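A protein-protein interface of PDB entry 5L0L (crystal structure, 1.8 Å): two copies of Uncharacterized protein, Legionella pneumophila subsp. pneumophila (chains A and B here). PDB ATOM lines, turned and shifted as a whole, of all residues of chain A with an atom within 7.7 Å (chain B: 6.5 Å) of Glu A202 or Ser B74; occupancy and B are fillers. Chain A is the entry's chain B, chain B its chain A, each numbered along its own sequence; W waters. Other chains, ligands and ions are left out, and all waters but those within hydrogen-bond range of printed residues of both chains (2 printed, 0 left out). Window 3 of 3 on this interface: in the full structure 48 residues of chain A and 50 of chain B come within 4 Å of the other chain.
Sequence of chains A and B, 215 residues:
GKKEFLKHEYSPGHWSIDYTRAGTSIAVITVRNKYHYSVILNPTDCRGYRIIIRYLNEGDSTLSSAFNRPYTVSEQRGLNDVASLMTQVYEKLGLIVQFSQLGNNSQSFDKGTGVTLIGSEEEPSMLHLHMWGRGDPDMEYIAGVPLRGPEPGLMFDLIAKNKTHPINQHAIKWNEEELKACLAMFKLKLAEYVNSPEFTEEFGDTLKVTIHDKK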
ATOM      1  N   SER A  84       8.416  -4.869   8.323  1.00  0.00           N
ATOM      2  CA  SER A  84       8.538  -5.329   9.721  1.00  0.00           C
ATOM      3  C   SER A  84       9.772  -6.211   9.922  1.00  0.00           C
ATOM      4  O   SER A  84      10.506  -6.033  10.891  1.00  0.00           O
ATOM      5  CB  SER A  84       7.290  -6.076  10.174  1.00  0.00           C
ATOM      6  OG  SER A  84       6.122  -5.272  10.039  1.00  0.00           O
ATOM      7  N   LEU A  85      10.020  -7.122   8.991  1.00  0.00           N
ATOM      8  CA  LEU A  85      11.240  -7.948   9.038  1.00  0.00           C
ATOM      9  C   LEU A  85      12.494  -7.097   8.967  1.00  0.00           C
ATOM     10  O   LEU A  85      13.397  -7.233   9.799  1.00  0.00           O
ATOM     11  CB  LEU A  85      11.243  -8.970   7.897  1.00  0.00           C
ATOM     12  CG  LEU A  85      12.557  -9.738   7.646  1.00  0.00           C
ATOM     13  CD1 LEU A  85      12.934 -10.548   8.865  1.00  0.00           C
ATOM     14  CD2 LEU A  85      12.412 -10.636   6.448  1.00  0.00           C
ATOM     15  N   GLN A  88      14.280  -5.219  11.928  1.00  0.00           N
ATOM     16  CA  GLN A  88      15.134  -5.973  12.861  1.00  0.00           C
ATOM     17  C   GLN A  88      16.605  -5.908  12.508  1.00  0.00           C
ATOM     18  O   GLN A  88      17.447  -5.956  13.403  1.00  0.00           O
ATOM     19  CB  GLN A  88      14.625  -7.426  13.036  1.00  0.00           C
ATOM     20  CG  GLN A  88      13.179  -7.436  13.525  1.00  0.00           C
ATOM     21  CD  GLN A  88      12.992  -6.596  14.786  1.00  0.00           C
ATOM     22  OE1 GLN A  88      13.542  -6.945  15.830  1.00  0.00           O
ATOM     23  NE2 GLN A  88      12.296  -5.458  14.684  1.00  0.00           N
ATOM     24  N   TYR A 193      19.233 -13.351  11.416  1.00  0.00           N
ATOM     25  CA  TYR A 193      17.869 -13.222  11.921  1.00  0.00           C
ATOM     26  C   TYR A 193      16.906 -14.272  11.359  1.00  0.00           C
ATOM     27  O   TYR A 193      16.100 -14.870  12.116  1.00  0.00           O
ATOM     28  CB  TYR A 193      17.334 -11.804  11.653  1.00  0.00           C
ATOM     29  CG  TYR A 193      16.032 -11.564  12.378  1.00  0.00           C
ATOM     30  CD1 TYR A 193      16.020 -11.422  13.764  1.00  0.00           C
ATOM     31  CD2 TYR A 193      14.808 -11.525  11.690  1.00  0.00           C
ATOM     32  CE1 TYR A 193      14.830 -11.241  14.464  1.00  0.00           C
ATOM     33  CE2 TYR A 193      13.608 -11.328  12.379  1.00  0.00           C
ATOM     34  CZ  TYR A 193      13.627 -11.177  13.765  1.00  0.00           C
ATOM     35  OH  TYR A 193      12.460 -11.008  14.484  1.00  0.00           O
ATOM     36  N   SER A 196      15.923 -17.885  12.808  1.00  0.00           N
ATOM     37  CA  SER A 196      16.278 -17.921  14.239  1.00  0.00           C
ATOM     38  C   SER A 196      14.984 -18.165  14.995  1.00  0.00           C
ATOM     39  O   SER A 196      13.917 -18.147  14.363  1.00  0.00           O
ATOM     40  CB  SER A 196      16.903 -16.597  14.693  1.00  0.00           C
ATOM     41  OG  SER A 196      15.984 -15.511  14.567  1.00  0.00           O
ATOM     42  N   PRO A 197      15.054 -18.405  16.334  1.00  0.00           N
ATOM     43  CA  PRO A 197      13.753 -18.725  16.973  1.00  0.00           C
ATOM     44  C   PRO A 197      12.725 -17.610  16.909  1.00  0.00           C
ATOM     45  O   PRO A 197      11.570 -17.880  16.613  1.00  0.00           O
ATOM     46  CB  PRO A 197      14.147 -19.022  18.428  1.00  0.00           C
ATOM     47  CG  PRO A 197      15.488 -19.655  18.287  1.00  0.00           C
ATOM     48  CD  PRO A 197      16.173 -18.850  17.198  1.00  0.00           C
ATOM     49  N   GLU A 198      13.178 -16.380  17.153  1.00  0.00           N
ATOM     50  CA  GLU A 198      12.341 -15.191  17.128  1.00  0.00           C
ATOM     51  C   GLU A 198      11.650 -14.952  15.781  1.00  0.00           C
ATOM     52  O   GLU A 198      10.497 -14.525  15.748  1.00  0.00           O
ATOM     53  CB  GLU A 198      13.187 -13.972  17.510  1.00  0.00           C
ATOM     54  CG  GLU A 198      13.790 -14.047  18.907  1.00  0.00           C
ATOM     55  CD  GLU A 198      15.188 -14.631  18.945  1.00  0.00           C
ATOM     56  OE1 GLU A 198      15.433 -15.772  18.477  1.00  0.00           O
ATOM     57  OE2 GLU A 198      16.060 -13.936  19.493  1.00  0.00           O
ATOM     58  N   PHE A 199      12.358 -15.224  14.681  1.00  0.00           N
ATOM     59  CA  PHE A 199      11.798 -15.094  13.317  1.00  0.00           C
ATOM     60  C   PHE A 199      10.726 -16.163  13.074  1.00  0.00           C
ATOM     61  O   PHE A 199       9.653 -15.860  12.558  1.00  0.00           O
ATOM     62  CB  PHE A 199      12.899 -15.187  12.253  1.00  0.00           C
ATOM     63  CG  PHE A 199      12.393 -15.264  10.830  1.00  0.00           C
ATOM     64  CD1 PHE A 199      11.996 -16.483  10.277  1.00  0.00           C
ATOM     65  CD2 PHE A 199      12.364 -14.136  10.022  1.00  0.00           C
ATOM     66  CE1 PHE A 199      11.558 -16.579   8.970  1.00  0.00           C
ATOM     67  CE2 PHE A 199      11.920 -14.219   8.712  1.00  0.00           C
ATOM     68  CZ  PHE A 199      11.521 -15.444   8.180  1.00  0.00           C
ATOM     69  N   THR A 200      11.037 -17.406  13.416  1.00  0.00           N
ATOM     70  CA  THR A 200      10.074 -18.480  13.252  1.00  0.00           C
ATOM     71  C   THR A 200       8.814 -18.225  14.088  1.00  0.00           C
ATOM     72  O   THR A 200       7.717 -18.384  13.575  1.00  0.00           O
ATOM     73  CB  THR A 200      10.692 -19.840  13.578  1.00  0.00           C
ATOM     74  OG1 THR A 200      11.850 -20.005  12.767  1.00  0.00           O
ATOM     75  CG2 THR A 200       9.700 -20.980  13.285  1.00  0.00           C
ATOM     76  N   GLU A 201       8.968 -17.778  15.330  1.00  0.00           N
ATOM     77  CA  GLU A 201       7.799 -17.419  16.183  1.00  0.00           C
ATOM     78  C   GLU A 201       6.867 -16.396  15.558  1.00  0.00           C
ATOM     79  O   GLU A 201       5.652 -16.504  15.678  1.00  0.00           O
ATOM     80  CB  GLU A 201       8.243 -16.834  17.532  1.00  0.00           C
ATOM     81  CG  GLU A 201       8.625 -17.857  18.597  1.00  0.00           C
ATOM     82  CD  GLU A 201       9.694 -17.353  19.581  1.00  0.00           C
ATOM     83  OE1 GLU A 201       9.825 -16.106  19.776  1.00  0.00           O
ATOM     84  OE2 GLU A 201      10.421 -18.223  20.148  1.00  0.00           O
ATOM     85  N   GLU A 202       7.437 -15.370  14.934  1.00  0.00           N
ATOM     86  CA  GLU A 202       6.654 -14.274  14.420  1.00  0.00           C
ATOM     87  C   GLU A 202       6.146 -14.506  13.008  1.00  0.00           C
ATOM     88  O   GLU A 202       4.997 -14.181  12.702  1.00  0.00           O
ATOM     89  CB  GLU A 202       7.476 -12.973  14.420  1.00  0.00           C
ATOM     90  CG  GLU A 202       6.643 -11.737  14.067  1.00  0.00           C
ATOM     91  CD  GLU A 202       5.445 -11.565  14.984  1.00  0.00           C
ATOM     92  OE1 GLU A 202       4.332 -11.210  14.509  1.00  0.00           O
ATOM     93  OE2 GLU A 202       5.637 -11.810  16.190  1.00  0.00           O
ATOM     94  N   PHE A 203       7.015 -14.986  12.136  1.00  0.00           N
ATOM     95  CA  PHE A 203       6.686 -15.081  10.722  1.00  0.00           C
ATOM     96  C   PHE A 203       6.307 -16.514  10.297  1.00  0.00           C
ATOM     97  O   PHE A 203       5.694 -16.710   9.248  1.00  0.00           O
ATOM     98  CB  PHE A 203       7.831 -14.506   9.897  1.00  0.00           C
ATOM     99  CG  PHE A 203       8.046 -13.015  10.125  1.00  0.00           C
ATOM    100  CD1 PHE A 203       7.118 -12.083   9.650  1.00  0.00           C
ATOM    101  CD2 PHE A 203       9.146 -12.550  10.836  1.00  0.00           C
ATOM    102  CE1 PHE A 203       7.312 -10.727   9.868  1.00  0.00           C
ATOM    103  CE2 PHE A 203       9.331 -11.197  11.075  1.00  0.00           C
ATOM    104  CZ  PHE A 203       8.416 -10.284  10.581  1.00  0.00           C
ATOM    105  N   GLY A 204       6.637 -17.496  11.128  1.00  0.00           N
ATOM    106  CA  GLY A 204       6.386 -18.902  10.798  1.00  0.00           C
ATOM    107  C   GLY A 204       6.921 -19.185   9.412  1.00  0.00           C
ATOM    108  O   GLY A 204       8.095 -18.991   9.157  1.00  0.00           O
ATOM    109  N   ASP A 205       6.004 -19.543   8.524  1.00  0.00           N
ATOM    110  CA  ASP A 205       6.266 -19.951   7.146  1.00  0.00           C
ATOM    111  C   ASP A 205       5.902 -18.821   6.149  1.00  0.00           C
ATOM    112  O   ASP A 205       6.135 -18.984   4.941  1.00  0.00           O
ATOM    113  CB  ASP A 205       5.375 -21.197   6.865  1.00  0.00           C
ATOM    114  CG  ASP A 205       6.067 -22.264   6.026  1.00  0.00           C
ATOM    115  OD1 ASP A 205       6.714 -21.922   5.012  1.00  0.00           O
ATOM    116  OD2 ASP A 205       5.935 -23.460   6.376  1.00  0.00           O
ATOM    117  N   THR A 206       5.344 -17.710   6.672  1.00  0.00           N
ATOM    118  CA  THR A 206       4.788 -16.570   5.925  1.00  0.00           C
ATOM    119  C   THR A 206       5.772 -15.935   4.938  1.00  0.00           C
ATOM    120  O   THR A 206       5.386 -15.563   3.826  1.00  0.00           O
ATOM    121  CB  THR A 206       4.375 -15.432   6.912  1.00  0.00           C
ATOM    122  OG1 THR A 206       3.493 -15.947   7.918  1.00  0.00           O
ATOM    123  CG2 THR A 206       3.670 -14.305   6.211  1.00  0.00           C
ATOM    124  N   LEU A 207       7.018 -15.769   5.382  1.00  0.00           N
ATOM    125  CA  LEU A 207       8.077 -15.106   4.593  1.00  0.00           C
ATOM    126  C   LEU A 207       9.149 -16.093   4.182  1.00  0.00           C
ATOM    127  O   LEU A 207       9.642 -16.809   5.040  1.00  0.00           O
ATOM    128  CB  LEU A 207       8.736 -14.011   5.419  1.00  0.00           C
ATOM    129  CG  LEU A 207       7.836 -12.885   5.932  1.00  0.00           C
ATOM    130  CD1 LEU A 207       8.637 -11.821   6.673  1.00  0.00           C
ATOM    131  CD2 LEU A 207       7.073 -12.270   4.790  1.00  0.00           C
ATOM    132  N   VAL B  31      -4.481  -6.678  17.660  1.00  0.00           N
ATOM    133  CA  VAL B  31      -3.813  -7.564  16.730  1.00  0.00           C
ATOM    134  C   VAL B  31      -3.490  -8.894  17.451  1.00  0.00           C
ATOM    135  O   VAL B  31      -2.857  -8.874  18.512  1.00  0.00           O
ATOM    136  CB  VAL B  31      -2.491  -6.966  16.221  1.00  0.00           C
ATOM    137  CG1 VAL B  31      -1.785  -7.930  15.273  1.00  0.00           C
ATOM    138  CG2 VAL B  31      -2.761  -5.653  15.497  1.00  0.00           C
ATOM    139  N   ARG B  32      -3.990 -10.002  16.882  1.00  0.00           N
ATOM    140  CA  ARG B  32      -3.692 -11.383  17.342  1.00  0.00           C
ATOM    141  C   ARG B  32      -4.068 -11.542  18.796  1.00  0.00           C
ATOM    142  O   ARG B  32      -3.325 -12.138  19.574  1.00  0.00           O
ATOM    143  CB  ARG B  32      -2.207 -11.732  17.113  1.00  0.00           C
ATOM    144  CG  ARG B  32      -1.825 -11.822  15.640  1.00  0.00           C
ATOM    145  CD  ARG B  32      -0.316 -11.768  15.359  1.00  0.00           C
ATOM    146  NE  ARG B  32      -0.144 -11.796  13.902  1.00  0.00           N
ATOM    147  CZ  ARG B  32       0.152 -10.759  13.099  1.00  0.00           C
ATOM    148  NH1 ARG B  32       0.459  -9.541  13.569  1.00  0.00           N
ATOM    149  NH2 ARG B  32       0.212 -10.970  11.776  1.00  0.00           N
ATOM    150  N   LYS B  34      -3.916  -9.649  21.360  1.00  0.00           N
ATOM    151  CA  LYS B  34      -2.870  -9.340  22.308  1.00  0.00           C
ATOM    152  C   LYS B  34      -2.342  -7.901  22.242  1.00  0.00           C
ATOM    153  O   LYS B  34      -2.157  -7.266  23.279  1.00  0.00           O
ATOM    154  CB  LYS B  34      -1.716 -10.318  22.095  1.00  0.00           C
ATOM    155  CG  LYS B  34      -0.680 -10.278  23.201  1.00  0.00           C
ATOM    156  CD  LYS B  34       0.412 -11.334  23.040  1.00  0.00           C
ATOM    157  CE  LYS B  34       1.645 -10.935  23.845  1.00  0.00           C
ATOM    158  NZ  LYS B  34       2.752 -11.920  23.710  1.00  0.00           N
ATOM    159  N   TYR B  35      -2.042  -7.414  21.040  1.00  0.00           N
ATOM    160  CA  TYR B  35      -1.407  -6.091  20.898  1.00  0.00           C
ATOM    161  C   TYR B  35      -2.469  -5.056  20.552  1.00  0.00           C
ATOM    162  O   TYR B  35      -3.218  -5.242  19.583  1.00  0.00           O
ATOM    163  CB  TYR B  35      -0.303  -6.138  19.854  1.00  0.00           C
ATOM    164  CG  TYR B  35       0.778  -7.144  20.197  1.00  0.00           C
ATOM    165  CD1 TYR B  35       1.795  -6.838  21.108  1.00  0.00           C
ATOM    166  CD2 TYR B  35       0.758  -8.427  19.641  1.00  0.00           C
ATOM    167  CE1 TYR B  35       2.780  -7.776  21.438  1.00  0.00           C
ATOM    168  CE2 TYR B  35       1.743  -9.371  19.961  1.00  0.00           C
ATOM    169  CZ  TYR B  35       2.741  -9.044  20.861  1.00  0.00           C
ATOM    170  OH  TYR B  35       3.695  -9.994  21.170  1.00  0.00           O
ATOM    171  N   TYR B  37      -3.745  -1.144  19.667  1.00  0.00           N
ATOM    172  CA  TYR B  37      -3.323   0.080  18.948  1.00  0.00           C
ATOM    173  C   TYR B  37      -4.473   1.080  18.856  1.00  0.00           C
ATOM    174  O   TYR B  37      -5.628   0.667  18.729  1.00  0.00           O
ATOM    175  CB  TYR B  37      -2.854  -0.278  17.527  1.00  0.00           C
ATOM    176  CG  TYR B  37      -1.698  -1.250  17.512  1.00  0.00           C
ATOM    177  CD1 TYR B  37      -1.926  -2.616  17.582  1.00  0.00           C
ATOM    178  CD2 TYR B  37      -0.383  -0.800  17.475  1.00  0.00           C
ATOM    179  CE1 TYR B  37      -0.881  -3.529  17.589  1.00  0.00           C
ATOM    180  CE2 TYR B  37       0.677  -1.707  17.493  1.00  0.00           C
ATOM    181  CZ  TYR B  37       0.418  -3.068  17.577  1.00  0.00           C
ATOM    182  OH  TYR B  37       1.461  -3.960  17.605  1.00  0.00           O
ATOM    183  N   TYR B  71      11.191  -1.910  20.974  1.00  0.00           N
ATOM    184  CA  TYR B  71       9.965  -2.599  20.615  1.00  0.00           C
ATOM    185  C   TYR B  71      10.336  -3.920  19.968  1.00  0.00           C
ATOM    186  O   TYR B  71      11.301  -4.020  19.213  1.00  0.00           O
ATOM    187  CB  TYR B  71       9.045  -1.712  19.706  1.00  0.00           C
ATOM    188  CG  TYR B  71       8.642  -0.482  20.461  1.00  0.00           C
ATOM    189  CD1 TYR B  71       7.749  -0.563  21.523  1.00  0.00           C
ATOM    190  CD2 TYR B  71       9.219   0.745  20.183  1.00  0.00           C
ATOM    191  CE1 TYR B  71       7.441   0.549  22.284  1.00  0.00           C
ATOM    192  CE2 TYR B  71       8.908   1.855  20.913  1.00  0.00           C
ATOM    193  CZ  TYR B  71       8.047   1.754  21.980  1.00  0.00           C
ATOM    194  OH  TYR B  71       7.771   2.876  22.716  1.00  0.00           O
ATOM    195  N   THR B  72       9.522  -4.916  20.255  1.00  0.00           N
ATOM    196  CA  THR B  72       9.727  -6.251  19.722  1.00  0.00           C
ATOM    197  C   THR B  72       9.242  -6.297  18.296  1.00  0.00           C
ATOM    198  O   THR B  72       8.450  -5.455  17.867  1.00  0.00           O
ATOM    199  CB  THR B  72       8.968  -7.315  20.541  1.00  0.00           C
ATOM    200  OG1 THR B  72       7.557  -7.202  20.337  1.00  0.00           O
ATOM    201  CG2 THR B  72       9.276  -7.175  22.028  1.00  0.00           C
ATOM    202  N   VAL B  73       9.695  -7.316  17.579  1.00  0.00           N
ATOM    203  CA  VAL B  73       9.216  -7.526  16.224  1.00  0.00           C
ATOM    204  C   VAL B  73       7.686  -7.717  16.172  1.00  0.00           C
ATOM    205  O   VAL B  73       7.052  -7.220  15.238  1.00  0.00           O
ATOM    206  CB  VAL B  73       9.968  -8.654  15.497  1.00  0.00           C
ATOM    207  CG1 VAL B  73       9.677 -10.027  16.095  1.00  0.00           C
ATOM    208  CG2 VAL B  73       9.630  -8.643  14.023  1.00  0.00           C
ATOM    209  N   SER B  74       7.086  -8.398  17.157  1.00  0.00           N
ATOM    210  CA  SER B  74       5.614  -8.532  17.156  1.00  0.00           C
ATOM    211  C   SER B  74       4.901  -7.180  17.288  1.00  0.00           C
ATOM    212  O   SER B  74       3.864  -6.968  16.658  1.00  0.00           O
ATOM    213  CB  SER B  74       5.110  -9.397  18.291  1.00  0.00           C
ATOM    214  OG  SER B  74       5.821 -10.614  18.281  1.00  0.00           O
ATOM    215  N   GLU B  75       5.441  -6.318  18.137  1.00  0.00           N
ATOM    216  CA  GLU B  75       4.872  -4.983  18.343  1.00  0.00           C
ATOM    217  C   GLU B  75       4.951  -4.161  17.064  1.00  0.00           C
ATOM    218  O   GLU B  75       3.965  -3.535  16.655  1.00  0.00           O
ATOM    219  CB  GLU B  75       5.564  -4.277  19.537  1.00  0.00           C
ATOM    220  CG  GLU B  75       5.215  -4.924  20.884  1.00  0.00           C
ATOM    221  CD  GLU B  75       6.071  -4.502  22.069  1.00  0.00           C
ATOM    222  OE1 GLU B  75       7.216  -4.022  21.893  1.00  0.00           O
ATOM    223  OE2 GLU B  75       5.575  -4.644  23.201  1.00  0.00           O
ATOM    224  N   GLN B  76       6.121  -4.166  16.432  1.00  0.00           N
ATOM    225  CA  GLN B  76       6.299  -3.476  15.155  1.00  0.00           C
ATOM    226  C   GLN B  76       5.412  -4.059  14.057  1.00  0.00           C
ATOM    227  O   GLN B  76       4.795  -3.332  13.245  1.00  0.00           O
ATOM    228  CB  GLN B  76       7.781  -3.510  14.740  1.00  0.00           C
ATOM    229  CG  GLN B  76       8.056  -2.871  13.374  1.00  0.00           C
ATOM    230  CD  GLN B  76       7.974  -1.348  13.434  1.00  0.00           C
ATOM    231  OE1 GLN B  76       6.966  -0.710  12.993  1.00  0.00           O
ATOM    232  NE2 GLN B  76       8.972  -0.758  14.004  1.00  0.00           N
ATOM    233  N   ARG B  77       5.355  -5.388  14.008  1.00  0.00           N
ATOM    234  CA  ARG B  77       4.555  -6.044  13.005  1.00  0.00           C
ATOM    235  C   ARG B  77       3.070  -5.674  13.134  1.00  0.00           C
ATOM    236  O   ARG B  77       2.390  -5.463  12.133  1.00  0.00           O
ATOM    237  CB  ARG B  77       4.717  -7.560  13.088  1.00  0.00           C
ATOM    238  CG  ARG B  77       4.216  -8.217  11.832  1.00  0.00           C
ATOM    239  CD  ARG B  77       4.095  -9.702  11.989  1.00  0.00           C
ATOM    240  NE  ARG B  77       3.757 -10.270  10.691  1.00  0.00           N
ATOM    241  CZ  ARG B  77       3.445 -11.538  10.506  1.00  0.00           C
ATOM    242  NH1 ARG B  77       3.173 -11.966   9.272  1.00  0.00           N
ATOM    243  NH2 ARG B  77       3.420 -12.362  11.535  1.00  0.00           N
ATOM    244  N   GLY B  78       2.586  -5.630  14.368  1.00  0.00           N
ATOM    245  CA  GLY B  78       1.192  -5.270  14.637  1.00  0.00           C
ATOM    246  C   GLY B  78       0.894  -3.828  14.209  1.00  0.00           C
ATOM    247  O   GLY B  78      -0.143  -3.580  13.629  1.00  0.00           O
ATOM    248  N   LEU B  79       1.806  -2.905  14.503  1.00  0.00           N
ATOM    249  CA  LEU B  79       1.669  -1.498  14.041  1.00  0.00           C
ATOM    250  C   LEU B  79       1.511  -1.478  12.534  1.00  0.00           C
ATOM    251  O   LEU B  79       0.628  -0.818  11.986  1.00  0.00           O
ATOM    252  CB  LEU B  79       2.879  -0.661  14.459  1.00  0.00           C
ATOM    253  CG  LEU B  79       2.718   0.846  14.229  1.00  0.00           C
ATOM    254  CD1 LEU B  79       1.818   1.441  15.284  1.00  0.00           C
ATOM    255  CD2 LEU B  79       4.027   1.590  14.236  1.00  0.00           C
ATOM    256  N   ASP B  81       0.613  -3.911  10.516  1.00  0.00           N
ATOM    257  CA  ASP B  81      -0.661  -4.520  10.086  1.00  0.00           C
ATOM    258  C   ASP B  81      -1.815  -3.509  10.195  1.00  0.00           C
ATOM    259  O   ASP B  81      -2.660  -3.417   9.297  1.00  0.00           O
ATOM    260  CB  ASP B  81      -1.001  -5.754  10.938  1.00  0.00           C
ATOM    261  CG  ASP B  81      -0.172  -6.982  10.591  1.00  0.00           C
ATOM    262  OD1 ASP B  81       0.532  -7.034   9.549  1.00  0.00           O
ATOM    263  OD2 ASP B  81      -0.249  -7.968  11.395  1.00  0.00           O
HETATM  264  O   HOH W   1       3.607  -6.234   9.360  1.00  0.00           O
HETATM  265  O   HOH W   2      12.041  -3.309  16.725  1.00  0.00           O
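NH2 of Arg B77 is in salt-bridge range of OE1 of Glu A202, at 3.3 Å. The side-chain carboxylate (OE2) of Glu A202 lies within hydrogen-bond range of the side-chain hydroxyl (OG) of Ser B74.
OG1 of Thr B72 lies close to N of Ser B74. OG1 of Thr A206 is in hydrogen-bond range of O of Phe A203, at 2.7 Å. The backbone carbonyl oxygen of Tyr A193 lies within hydrogen-bond range of the side-chain hydroxyl of Ser A196 (2.5 Å).
Gln B76 touches Ser A84 (O to OG, 3.98 Å). Ser A84 touches Arg B77. Gln A88 touches Val B73 (CD to CB, 3.7 Å). Tyr A193 touches Val B73. CG2 of Val B73 touches CE2 of Phe A203 (3.9 Å). Arg B77 touches Phe A203 (NE to CE1, 3.7 Å). Thr A206 touches Arg B77.
Of the printed residues of chain B, Ser A84 touches Gln B76 (3.98 Å) and Arg B77 (3.4 Å). Printed residues of chain B within 4 Å of Tyr A193: Val B73 (3.4 Å). Phe A199 touches none of the printed residues of chain B. Glu A202 touches two residues of chain B. Of the printed residues of chain B, Phe A203 touches Val B73 (3.9 Å) and Arg B77 (3.7 Å). Printed residues of chain A within 4 Å of Arg B77: Ser A84, Glu A202, Phe A203 and Thr A206. The nearest printed residue of chain B that does not touch Phe A203 is Ser B74 (7.0 Å).
Printed residues of chain A that touch a printed residue of chain B: Ser A84, Gln A88, Tyr A193, Glu A202, Phe A203 and Thr A206. Printed residues of chain B that touch a printed residue of chain A: Val B73, Ser B74, Gln B76 and Arg B77. Among the printed residues, 9 pairs touch across the chains. Among the printed residues, Asp or Glu carboxylates within 4 Å of a Lys or Arg side-chain nitrogen of the other chain: Glu A202 with Arg B77 (3.3 Å).
No position is printed for both chains.
Water W2 lies within hydrogen-bond range of O of Tyr B71 (2.7 Å) and NE2 of Gln A88 (3.0 Å). Water W1 lies within hydrogen-bond range of the side-chain hydroxyl of Ser A84 (2.8 Å), the backbone carbonyl oxygen of Arg B77 (3.1 Å) and the side-chain carboxylate of Asp B81 (3.2 Å).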
